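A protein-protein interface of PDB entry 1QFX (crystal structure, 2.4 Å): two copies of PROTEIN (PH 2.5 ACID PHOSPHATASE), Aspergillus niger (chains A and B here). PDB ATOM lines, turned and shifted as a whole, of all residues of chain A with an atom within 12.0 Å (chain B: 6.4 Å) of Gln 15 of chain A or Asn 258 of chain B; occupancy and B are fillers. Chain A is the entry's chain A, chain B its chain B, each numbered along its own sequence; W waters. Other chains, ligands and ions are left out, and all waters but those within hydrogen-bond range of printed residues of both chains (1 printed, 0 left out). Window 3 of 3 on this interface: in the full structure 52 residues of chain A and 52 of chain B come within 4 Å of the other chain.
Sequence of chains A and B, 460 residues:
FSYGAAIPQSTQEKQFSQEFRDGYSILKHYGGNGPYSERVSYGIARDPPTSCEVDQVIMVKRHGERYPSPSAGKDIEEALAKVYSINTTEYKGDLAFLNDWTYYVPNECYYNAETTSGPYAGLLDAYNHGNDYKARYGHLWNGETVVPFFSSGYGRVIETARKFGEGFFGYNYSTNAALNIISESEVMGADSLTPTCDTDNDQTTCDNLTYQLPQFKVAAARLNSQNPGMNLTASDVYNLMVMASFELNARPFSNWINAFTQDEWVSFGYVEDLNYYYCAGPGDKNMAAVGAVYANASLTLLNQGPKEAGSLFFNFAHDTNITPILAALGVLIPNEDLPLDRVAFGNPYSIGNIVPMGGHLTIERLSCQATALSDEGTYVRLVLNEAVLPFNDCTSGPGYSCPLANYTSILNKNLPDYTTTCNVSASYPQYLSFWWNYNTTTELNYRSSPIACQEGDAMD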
ATOM      1  N   LYS A  14      36.693 -21.377  -6.144  1.00  0.00           N
ATOM      2  CA  LYS A  14      35.201 -21.361  -5.945  1.00  0.00           C
ATOM      3  C   LYS A  14      34.591 -19.995  -5.676  1.00  0.00           C
ATOM      4  O   LYS A  14      35.237 -19.112  -5.147  1.00  0.00           O
ATOM      5  CB  LYS A  14      34.749 -22.352  -4.873  1.00  0.00           C
ATOM      6  CG  LYS A  14      35.323 -22.171  -3.507  1.00  0.00           C
ATOM      7  CD  LYS A  14      34.745 -23.220  -2.571  1.00  0.00           C
ATOM      8  CE  LYS A  14      35.406 -23.185  -1.216  1.00  0.00           C
ATOM      9  NZ  LYS A  14      34.626 -24.028  -0.284  1.00  0.00           N
ATOM     10  N   GLN A  15      33.304 -19.869  -5.966  1.00  0.00           N
ATOM     11  CA  GLN A  15      32.591 -18.608  -5.868  1.00  0.00           C
ATOM     12  C   GLN A  15      32.304 -18.044  -4.495  1.00  0.00           C
ATOM     13  O   GLN A  15      32.353 -16.834  -4.323  1.00  0.00           O
ATOM     14  CB  GLN A  15      31.281 -18.711  -6.668  1.00  0.00           C
ATOM     15  CG  GLN A  15      30.616 -17.385  -7.027  1.00  0.00           C
ATOM     16  CD  GLN A  15      29.532 -17.546  -8.082  1.00  0.00           C
ATOM     17  OE1 GLN A  15      29.075 -18.659  -8.336  1.00  0.00           O
ATOM     18  NE2 GLN A  15      29.160 -16.443  -8.749  1.00  0.00           N
ATOM     19  N   PHE A  16      31.924 -18.893  -3.544  1.00  0.00           N
ATOM     20  CA  PHE A  16      31.595 -18.441  -2.203  1.00  0.00           C
ATOM     21  C   PHE A  16      32.260 -19.289  -1.128  1.00  0.00           C
ATOM     22  O   PHE A  16      32.425 -20.502  -1.299  1.00  0.00           O
ATOM     23  CB  PHE A  16      30.092 -18.511  -2.000  1.00  0.00           C
ATOM     24  CG  PHE A  16      29.313 -17.726  -2.987  1.00  0.00           C
ATOM     25  CD1 PHE A  16      29.134 -16.354  -2.816  1.00  0.00           C
ATOM     26  CD2 PHE A  16      28.729 -18.353  -4.083  1.00  0.00           C
ATOM     27  CE1 PHE A  16      28.384 -15.619  -3.721  1.00  0.00           C
ATOM     28  CE2 PHE A  16      27.977 -17.626  -4.994  1.00  0.00           C
ATOM     29  CZ  PHE A  16      27.805 -16.251  -4.813  1.00  0.00           C
ATOM     30  N   SER A  17      32.620 -18.652  -0.010  1.00  0.00           N
ATOM     31  CA  SER A  17      33.241 -19.344   1.120  1.00  0.00           C
ATOM     32  C   SER A  17      32.119 -19.997   1.922  1.00  0.00           C
ATOM     33  O   SER A  17      31.037 -19.420   2.051  1.00  0.00           O
ATOM     34  CB  SER A  17      33.982 -18.352   2.016  1.00  0.00           C
ATOM     35  OG  SER A  17      34.476 -18.993   3.181  1.00  0.00           O
ATOM     36  N   GLN A  18      32.363 -21.197   2.443  1.00  0.00           N
ATOM     37  CA  GLN A  18      31.343 -21.897   3.231  1.00  0.00           C
ATOM     38  C   GLN A  18      31.477 -21.678   4.737  1.00  0.00           C
ATOM     39  O   GLN A  18      30.645 -22.135   5.508  1.00  0.00           O
ATOM     40  CB  GLN A  18      31.350 -23.385   2.900  1.00  0.00           C
ATOM     41  CG  GLN A  18      30.934 -23.677   1.457  1.00  0.00           C
ATOM     42  CD  GLN A  18      31.202 -25.110   1.036  1.00  0.00           C
ATOM     43  OE1 GLN A  18      32.334 -25.456   0.723  1.00  0.00           O
ATOM     44  NE2 GLN A  18      30.166 -25.938   0.999  1.00  0.00           N
ATOM     45  N   GLU A  19      32.519 -20.953   5.133  1.00  0.00           N
ATOM     46  CA  GLU A  19      32.791 -20.640   6.531  1.00  0.00           C
ATOM     47  C   GLU A  19      32.074 -19.330   6.890  1.00  0.00           C
ATOM     48  O   GLU A  19      32.147 -18.363   6.136  1.00  0.00           O
ATOM     49  CB  GLU A  19      34.289 -20.469   6.726  1.00  0.00           C
ATOM     50  CG  GLU A  19      35.140 -21.645   6.239  1.00  0.00           C
ATOM     51  CD  GLU A  19      36.569 -21.591   6.802  1.00  0.00           C
ATOM     52  OE1 GLU A  19      37.075 -20.467   7.050  1.00  0.00           O
ATOM     53  OE2 GLU A  19      37.196 -22.664   7.020  1.00  0.00           O
ATOM     54  N   PHE A  20      31.346 -19.311   8.005  1.00  0.00           N
ATOM     55  CA  PHE A  20      30.613 -18.131   8.450  1.00  0.00           C
ATOM     56  C   PHE A  20      30.998 -17.871   9.889  1.00  0.00           C
ATOM     57  O   PHE A  20      30.384 -18.383  10.829  1.00  0.00           O
ATOM     58  CB  PHE A  20      29.108 -18.350   8.291  1.00  0.00           C
ATOM     59  CG  PHE A  20      28.649 -18.202   6.876  1.00  0.00           C
ATOM     60  CD1 PHE A  20      28.979 -19.166   5.921  1.00  0.00           C
ATOM     61  CD2 PHE A  20      28.038 -17.029   6.453  1.00  0.00           C
ATOM     62  CE1 PHE A  20      28.723 -18.956   4.579  1.00  0.00           C
ATOM     63  CE2 PHE A  20      27.779 -16.812   5.108  1.00  0.00           C
ATOM     64  CZ  PHE A  20      28.127 -17.773   4.170  1.00  0.00           C
ATOM     65  N   ALA A  45      21.350  -4.876  -0.933  1.00  0.00           N
ATOM     66  CA  ALA A  45      22.425  -4.064  -1.501  1.00  0.00           C
ATOM     67  C   ALA A  45      22.428  -2.658  -0.870  1.00  0.00           C
ATOM     68  O   ALA A  45      21.382  -2.021  -0.735  1.00  0.00           O
ATOM     69  CB  ALA A  45      22.279  -3.983  -3.013  1.00  0.00           C
ATOM     70  N   THR A  50      18.685   0.375  -8.753  1.00  0.00           N
ATOM     71  CA  THR A  50      18.686   0.845 -10.136  1.00  0.00           C
ATOM     72  C   THR A  50      17.384   1.647 -10.291  1.00  0.00           C
ATOM     73  O   THR A  50      16.360   1.253  -9.707  1.00  0.00           O
ATOM     74  CB  THR A  50      18.697  -0.348 -11.081  1.00  0.00           C
ATOM     75  OG1 THR A  50      20.005  -0.916 -11.065  1.00  0.00           O
ATOM     76  CG2 THR A  50      18.350   0.059 -12.501  1.00  0.00           C
ATOM     77  N   ASP B  94      24.223  -9.257 -19.322  1.00  0.00           N
ATOM     78  CA  ASP B  94      24.514 -10.244 -18.293  1.00  0.00           C
ATOM     79  C   ASP B  94      24.400 -11.683 -18.776  1.00  0.00           C
ATOM     80  O   ASP B  94      24.959 -12.579 -18.155  1.00  0.00           O
ATOM     81  CB  ASP B  94      23.632 -10.016 -17.072  1.00  0.00           C
ATOM     82  CG  ASP B  94      23.808  -8.634 -16.489  1.00  0.00           C
ATOM     83  OD1 ASP B  94      24.905  -8.075 -16.614  1.00  0.00           O
ATOM     84  OD2 ASP B  94      22.846  -8.083 -15.926  1.00  0.00           O
ATOM     85  N   PRO B 119      34.007 -28.074  -6.209  1.00  0.00           N
ATOM     86  CA  PRO B 119      34.320 -27.963  -4.772  1.00  0.00           C
ATOM     87  C   PRO B 119      33.124 -28.215  -3.866  1.00  0.00           C
ATOM     88  O   PRO B 119      33.287 -28.449  -2.670  1.00  0.00           O
ATOM     89  CB  PRO B 119      34.809 -26.518  -4.641  1.00  0.00           C
ATOM     90  CG  PRO B 119      33.992 -25.780  -5.691  1.00  0.00           C
ATOM     91  CD  PRO B 119      34.055 -26.754  -6.874  1.00  0.00           C
ATOM     92  N   TYR B 120      31.926 -28.129  -4.439  1.00  0.00           N
ATOM     93  CA  TYR B 120      30.681 -28.310  -3.695  1.00  0.00           C
ATOM     94  C   TYR B 120      29.998 -29.660  -3.962  1.00  0.00           C
ATOM     95  O   TYR B 120      28.830 -29.861  -3.577  1.00  0.00           O
ATOM     96  CB  TYR B 120      29.692 -27.191  -4.035  1.00  0.00           C
ATOM     97  CG  TYR B 120      30.206 -25.768  -3.846  1.00  0.00           C
ATOM     98  CD1 TYR B 120      30.368 -25.212  -2.571  1.00  0.00           C
ATOM     99  CD2 TYR B 120      30.457 -24.958  -4.945  1.00  0.00           C
ATOM    100  CE1 TYR B 120      30.758 -23.871  -2.409  1.00  0.00           C
ATOM    101  CE2 TYR B 120      30.842 -23.624  -4.795  1.00  0.00           C
ATOM    102  CZ  TYR B 120      30.985 -23.091  -3.530  1.00  0.00           C
ATOM    103  OH  TYR B 120      31.308 -21.771  -3.402  1.00  0.00           O
ATOM    104  N   ALA B 244      20.115 -21.565 -11.146  1.00  0.00           N
ATOM    105  CA  ALA B 244      21.387 -20.954 -10.770  1.00  0.00           C
ATOM    106  C   ALA B 244      21.871 -21.449  -9.409  1.00  0.00           C
ATOM    107  O   ALA B 244      23.050 -21.758  -9.245  1.00  0.00           O
ATOM    108  CB  ALA B 244      21.273 -19.436 -10.767  1.00  0.00           C
ATOM    109  N   LEU B 248      25.853 -24.439  -8.521  1.00  0.00           N
ATOM    110  CA  LEU B 248      27.005 -24.515  -7.618  1.00  0.00           C
ATOM    111  C   LEU B 248      27.214 -25.942  -7.148  1.00  0.00           C
ATOM    112  O   LEU B 248      28.345 -26.354  -6.905  1.00  0.00           O
ATOM    113  CB  LEU B 248      26.816 -23.580  -6.405  1.00  0.00           C
ATOM    114  CG  LEU B 248      26.891 -22.063  -6.614  1.00  0.00           C
ATOM    115  CD1 LEU B 248      26.609 -21.346  -5.332  1.00  0.00           C
ATOM    116  CD2 LEU B 248      28.261 -21.683  -7.112  1.00  0.00           C
ATOM    117  N   ARG B 251      29.298 -27.183 -10.040  1.00  0.00           N
ATOM    118  CA  ARG B 251      30.400 -26.340 -10.511  1.00  0.00           C
ATOM    119  C   ARG B 251      30.898 -25.355  -9.456  1.00  0.00           C
ATOM    120  O   ARG B 251      30.141 -24.931  -8.584  1.00  0.00           O
ATOM    121  CB  ARG B 251      29.927 -25.552 -11.746  1.00  0.00           C
ATOM    122  CG  ARG B 251      29.668 -26.404 -12.977  1.00  0.00           C
ATOM    123  CD  ARG B 251      28.807 -25.706 -14.002  1.00  0.00           C
ATOM    124  NE  ARG B 251      28.770 -26.460 -15.257  1.00  0.00           N
ATOM    125  CZ  ARG B 251      27.999 -26.146 -16.293  1.00  0.00           C
ATOM    126  NH1 ARG B 251      27.185 -25.091 -16.229  1.00  0.00           N
ATOM    127  NH2 ARG B 251      28.039 -26.887 -17.386  1.00  0.00           N
ATOM    128  N   PRO B 252      32.163 -24.928  -9.566  1.00  0.00           N
ATOM    129  CA  PRO B 252      32.732 -23.977  -8.603  1.00  0.00           C
ATOM    130  C   PRO B 252      32.149 -22.559  -8.640  1.00  0.00           C
ATOM    131  O   PRO B 252      32.094 -21.885  -7.605  1.00  0.00           O
ATOM    132  CB  PRO B 252      34.223 -23.988  -8.945  1.00  0.00           C
ATOM    133  CG  PRO B 252      34.237 -24.339 -10.434  1.00  0.00           C
ATOM    134  CD  PRO B 252      33.188 -25.414 -10.515  1.00  0.00           C
ATOM    135  N   PHE B 253      31.731 -22.099  -9.820  1.00  0.00           N
ATOM    136  CA  PHE B 253      31.169 -20.753  -9.979  1.00  0.00           C
ATOM    137  C   PHE B 253      29.898 -20.887 -10.832  1.00  0.00           C
ATOM    138  O   PHE B 253      29.726 -21.877 -11.528  1.00  0.00           O
ATOM    139  CB  PHE B 253      32.182 -19.780 -10.695  1.00  0.00           C
ATOM    140  CG  PHE B 253      33.638 -19.821 -10.139  1.00  0.00           C
ATOM    141  CD1 PHE B 253      34.589 -20.755 -10.632  1.00  0.00           C
ATOM    142  CD2 PHE B 253      34.061 -18.931  -9.139  1.00  0.00           C
ATOM    143  CE1 PHE B 253      35.940 -20.809 -10.137  1.00  0.00           C
ATOM    144  CE2 PHE B 253      35.402 -18.980  -8.641  1.00  0.00           C
ATOM    145  CZ  PHE B 253      36.336 -19.923  -9.145  1.00  0.00           C
ATOM    146  N   SER B 254      28.975 -19.946 -10.709  1.00  0.00           N
ATOM    147  CA  SER B 254      27.793 -19.925 -11.542  1.00  0.00           C
ATOM    148  C   SER B 254      27.574 -18.482 -12.055  1.00  0.00           C
ATOM    149  O   SER B 254      27.293 -17.568 -11.268  1.00  0.00           O
ATOM    150  CB  SER B 254      26.562 -20.371 -10.769  1.00  0.00           C
ATOM    151  OG  SER B 254      25.395 -20.075 -11.527  1.00  0.00           O
ATOM    152  N   ASN B 255      27.701 -18.267 -13.361  1.00  0.00           N
ATOM    153  CA  ASN B 255      27.470 -16.934 -13.921  1.00  0.00           C
ATOM    154  C   ASN B 255      26.006 -16.551 -13.881  1.00  0.00           C
ATOM    155  O   ASN B 255      25.676 -15.378 -13.882  1.00  0.00           O
ATOM    156  CB  ASN B 255      27.984 -16.818 -15.349  1.00  0.00           C
ATOM    157  CG  ASN B 255      29.477 -16.906 -15.421  1.00  0.00           C
ATOM    158  OD1 ASN B 255      30.173 -16.430 -14.525  1.00  0.00           O
ATOM    159  ND2 ASN B 255      29.987 -17.569 -16.450  1.00  0.00           N
ATOM    160  N   TRP B 256      25.122 -17.537 -13.840  1.00  0.00           N
ATOM    161  CA  TRP B 256      23.697 -17.250 -13.761  1.00  0.00           C
ATOM    162  C   TRP B 256      23.357 -16.535 -12.458  1.00  0.00           C
ATOM    163  O   TRP B 256      22.391 -15.777 -12.389  1.00  0.00           O
ATOM    164  CB  TRP B 256      22.890 -18.541 -13.847  1.00  0.00           C
ATOM    165  CG  TRP B 256      22.507 -18.904 -15.247  1.00  0.00           C
ATOM    166  CD1 TRP B 256      23.089 -19.864 -16.043  1.00  0.00           C
ATOM    167  CD2 TRP B 256      21.441 -18.328 -16.016  1.00  0.00           C
ATOM    168  NE1 TRP B 256      22.439 -19.915 -17.258  1.00  0.00           N
ATOM    169  CE2 TRP B 256      21.426 -18.987 -17.268  1.00  0.00           C
ATOM    170  CE3 TRP B 256      20.495 -17.316 -15.770  1.00  0.00           C
ATOM    171  CZ2 TRP B 256      20.500 -18.668 -18.271  1.00  0.00           C
ATOM    172  CZ3 TRP B 256      19.567 -16.996 -16.772  1.00  0.00           C
ATOM    173  CH2 TRP B 256      19.579 -17.672 -18.003  1.00  0.00           C
ATOM    174  N   ILE B 257      24.129 -16.808 -11.410  1.00  0.00           N
ATOM    175  CA  ILE B 257      23.879 -16.177 -10.126  1.00  0.00           C
ATOM    176  C   ILE B 257      24.082 -14.685 -10.298  1.00  0.00           C
ATOM    177  O   ILE B 257      23.325 -13.879  -9.763  1.00  0.00           O
ATOM    178  CB  ILE B 257      24.813 -16.750  -9.001  1.00  0.00           C
ATOM    179  CG1 ILE B 257      24.285 -18.123  -8.550  1.00  0.00           C
ATOM    180  CG2 ILE B 257      24.948 -15.738  -7.802  1.00  0.00           C
ATOM    181  CD1 ILE B 257      25.144 -18.811  -7.503  1.00  0.00           C
ATOM    182  N   ASN B 258      25.079 -14.336 -11.101  1.00  0.00           N
ATOM    183  CA  ASN B 258      25.424 -12.946 -11.366  1.00  0.00           C
ATOM    184  C   ASN B 258      24.415 -12.178 -12.230  1.00  0.00           C
ATOM    185  O   ASN B 258      24.469 -10.954 -12.281  1.00  0.00           O
ATOM    186  CB  ASN B 258      26.810 -12.869 -12.007  1.00  0.00           C
ATOM    187  CG  ASN B 258      27.914 -13.296 -11.058  1.00  0.00           C
ATOM    188  OD1 ASN B 258      27.843 -13.034  -9.870  1.00  0.00           O
ATOM    189  ND2 ASN B 258      28.921 -13.971 -11.575  1.00  0.00           N
ATOM    190  N   ALA B 259      23.509 -12.881 -12.906  1.00  0.00           N
ATOM    191  CA  ALA B 259      22.517 -12.238 -13.763  1.00  0.00           C
ATOM    192  C   ALA B 259      21.357 -11.651 -12.956  1.00  0.00           C
ATOM    193  O   ALA B 259      20.475 -10.972 -13.505  1.00  0.00           O
ATOM    194  CB  ALA B 259      21.996 -13.231 -14.798  1.00  0.00           C
ATOM    195  N   PHE B 260      21.310 -11.972 -11.667  1.00  0.00           N
ATOM    196  CA  PHE B 260      20.261 -11.461 -10.792  1.00  0.00           C
ATOM    197  C   PHE B 260      20.928 -10.561  -9.757  1.00  0.00           C
ATOM    198  O   PHE B 260      22.132 -10.641  -9.532  1.00  0.00           O
ATOM    199  CB  PHE B 260      19.468 -12.601 -10.146  1.00  0.00           C
ATOM    200  CG  PHE B 260      18.892 -13.562 -11.153  1.00  0.00           C
ATOM    201  CD1 PHE B 260      17.696 -13.276 -11.807  1.00  0.00           C
ATOM    202  CD2 PHE B 260      19.586 -14.726 -11.506  1.00  0.00           C
ATOM    203  CE1 PHE B 260      17.203 -14.133 -12.814  1.00  0.00           C
ATOM    204  CE2 PHE B 260      19.099 -15.588 -12.508  1.00  0.00           C
ATOM    205  CZ  PHE B 260      17.907 -15.288 -13.163  1.00  0.00           C
ATOM    206  N   THR B 261      20.165  -9.625  -9.221  1.00  0.00           N
ATOM    207  CA  THR B 261      20.691  -8.695  -8.253  1.00  0.00           C
ATOM    208  C   THR B 261      20.673  -9.285  -6.846  1.00  0.00           C
ATOM    209  O   THR B 261      20.005 -10.292  -6.574  1.00  0.00           O
ATOM    210  CB  THR B 261      19.888  -7.322  -8.260  1.00  0.00           C
ATOM    211  OG1 THR B 261      18.529  -7.544  -7.859  1.00  0.00           O
ATOM    212  CG2 THR B 261      19.905  -6.668  -9.657  1.00  0.00           C
ATOM    213  N   TRP B 265      18.003 -12.049  -5.132  1.00  0.00           N
ATOM    214  CA  TRP B 265      18.406 -13.213  -4.364  1.00  0.00           C
ATOM    215  C   TRP B 265      17.807 -13.171  -2.945  1.00  0.00           C
ATOM    216  O   TRP B 265      17.328 -14.182  -2.441  1.00  0.00           O
ATOM    217  CB  TRP B 265      19.922 -13.308  -4.331  1.00  0.00           C
ATOM    218  CG  TRP B 265      20.439 -13.933  -5.572  1.00  0.00           C
ATOM    219  CD1 TRP B 265      21.191 -13.350  -6.533  1.00  0.00           C
ATOM    220  CD2 TRP B 265      20.220 -15.285  -5.992  1.00  0.00           C
ATOM    221  NE1 TRP B 265      21.465 -14.252  -7.541  1.00  0.00           N
ATOM    222  CE2 TRP B 265      20.876 -15.448  -7.233  1.00  0.00           C
ATOM    223  CE3 TRP B 265      19.534 -16.380  -5.435  1.00  0.00           C
ATOM    224  CZ2 TRP B 265      20.869 -16.661  -7.929  1.00  0.00           C
ATOM    225  CZ3 TRP B 265      19.526 -17.588  -6.131  1.00  0.00           C
ATOM    226  CH2 TRP B 265      20.190 -17.715  -7.365  1.00  0.00           C
HETATM  227  O   HOH W   1      30.463 -13.741  -8.452  1.00  0.00           O
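N of Gln 15 of chain A lies within hydrogen-bond range of O of Pro 252 of chain B (2.9 Å).
N of Ser 254 of chain B is in hydrogen-bond range of OE1 of Gln 15 of chain A.
The side-chain hydroxyl (OH) of Tyr 120 of chain B lies within hydrogen-bond range of the backbone carbonyl oxygen (O) of Phe 16 of chain A.
The side-chain amide oxygen (OE1) of Gln 18 of chain A sits at hydrogen-bond distance from the side-chain amino group (NZ) of Lys 14 of chain A (2.9 Å).
The backbone NH (N) of Trp 256 of chain B sits close to the side-chain hydroxyl (OG) of Ser 254 of chain B, 3.4 Å away.
The indole nitrogen (NE1) of Trp 265 of chain B is in hydrogen-bond range of the backbone carbonyl oxygen (O) of Ile 257 of chain B, at 2.9 Å.
Among the printed residues, pairs that only touch across the chains: Lys 14 of chain A with Pro 119 of chain B, Lys 14 of chain A with Tyr 120 of chain B, Lys 14 of chain A with Pro 252 of chain B, Lys 14 of chain A with Phe 253 of chain B, Gln 15 of chain A with Tyr 120 of chain B, Gln 15 of chain A with Leu 248 of chain B, Gln 15 of chain A with Phe 253 of chain B, Gln 15 of chain A with Asn 258 of chain B, Phe 16 of chain A with Leu 248 of chain B, Phe 16 of chain A with Ile 257 of chain B and Gln 18 of chain A with Tyr 120 of chain B.
Of chain B, only Tyr 120 (3.8 Å), Leu 248 (3.4 Å), Pro 252 (2.9 Å), Phe 253 (3.4 Å), Ser 254 (2.7 Å) and Asn 258 (3.8 Å) come within 4 Å of Gln 15 of chain A.
Asn 258 of chain B touches just one residue of chain A: Gln 15 (3.8 Å).
No residue of chain A comes within 4 Å of Asp 94 of chain B.
Of chain A, only Lys 14 and Gln 15 come within 4 Å of Pro 252 of chain B.
Phe 253 of chain B touches two residues of chain A.
Ser 254 of chain B touches just one residue of chain A: Gln 15 (2.7 Å).
No residue of chain A comes within 4 Å of Asn 255 of chain B.
Ile 257 of chain B touches just one residue of chain A: Phe 16 (3.97 Å).
Printed residues of chain B within 4 Å of Phe 16 of chain A: Tyr 120, Leu 248 and Ile 257.
Of the printed residues of chain B, Lys 14 of chain A touches Pro 119, Tyr 120, Pro 252 and Phe 253.
Of the printed residues of chain A, Tyr 120 of chain B touches Lys 14, Gln 15, Phe 16 and Gln 18.
Ser 17 of chain A touches none of the printed residues of chain B.
Glu 19 of chain A touches none of the printed residues of chain B.
The nearest residue of chain B that does not touch Gln 15 of chain A is Ile 257 of chain B (4.02 Å).
The nearest residue of chain A that does not touch Asn 258 of chain B is Phe 16 of chain A (6.0 Å).
Hydrophobic or aromatic side chains of chain B within 4 Å of the printed part of chain A: Pro 119, Tyr 120, Leu 248, Phe 253 and Ile 257.
Of the 9 printed residues of chain A, 4 touch a printed residue of chain B.
Printed residues of chain A that touch a printed residue of chain B: Lys 14, Gln 15, Phe 16 and Gln 18.
Hydrophobic or aromatic side chains of chain A within 4 Å of the printed part of chain B: Phe 16.
No position is printed for both chains.
Of the 14 pairs that touch across the chains among the printed residues, none has its exchanged pair printed and touching as well.
Water W1 lies within hydrogen-bond range of the side-chain amide nitrogen (NE2) of Gln 15 of chain A (3.0 Å) and the side-chain amide oxygen (OD1) of Asn 258 of chain B (3.1 Å).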
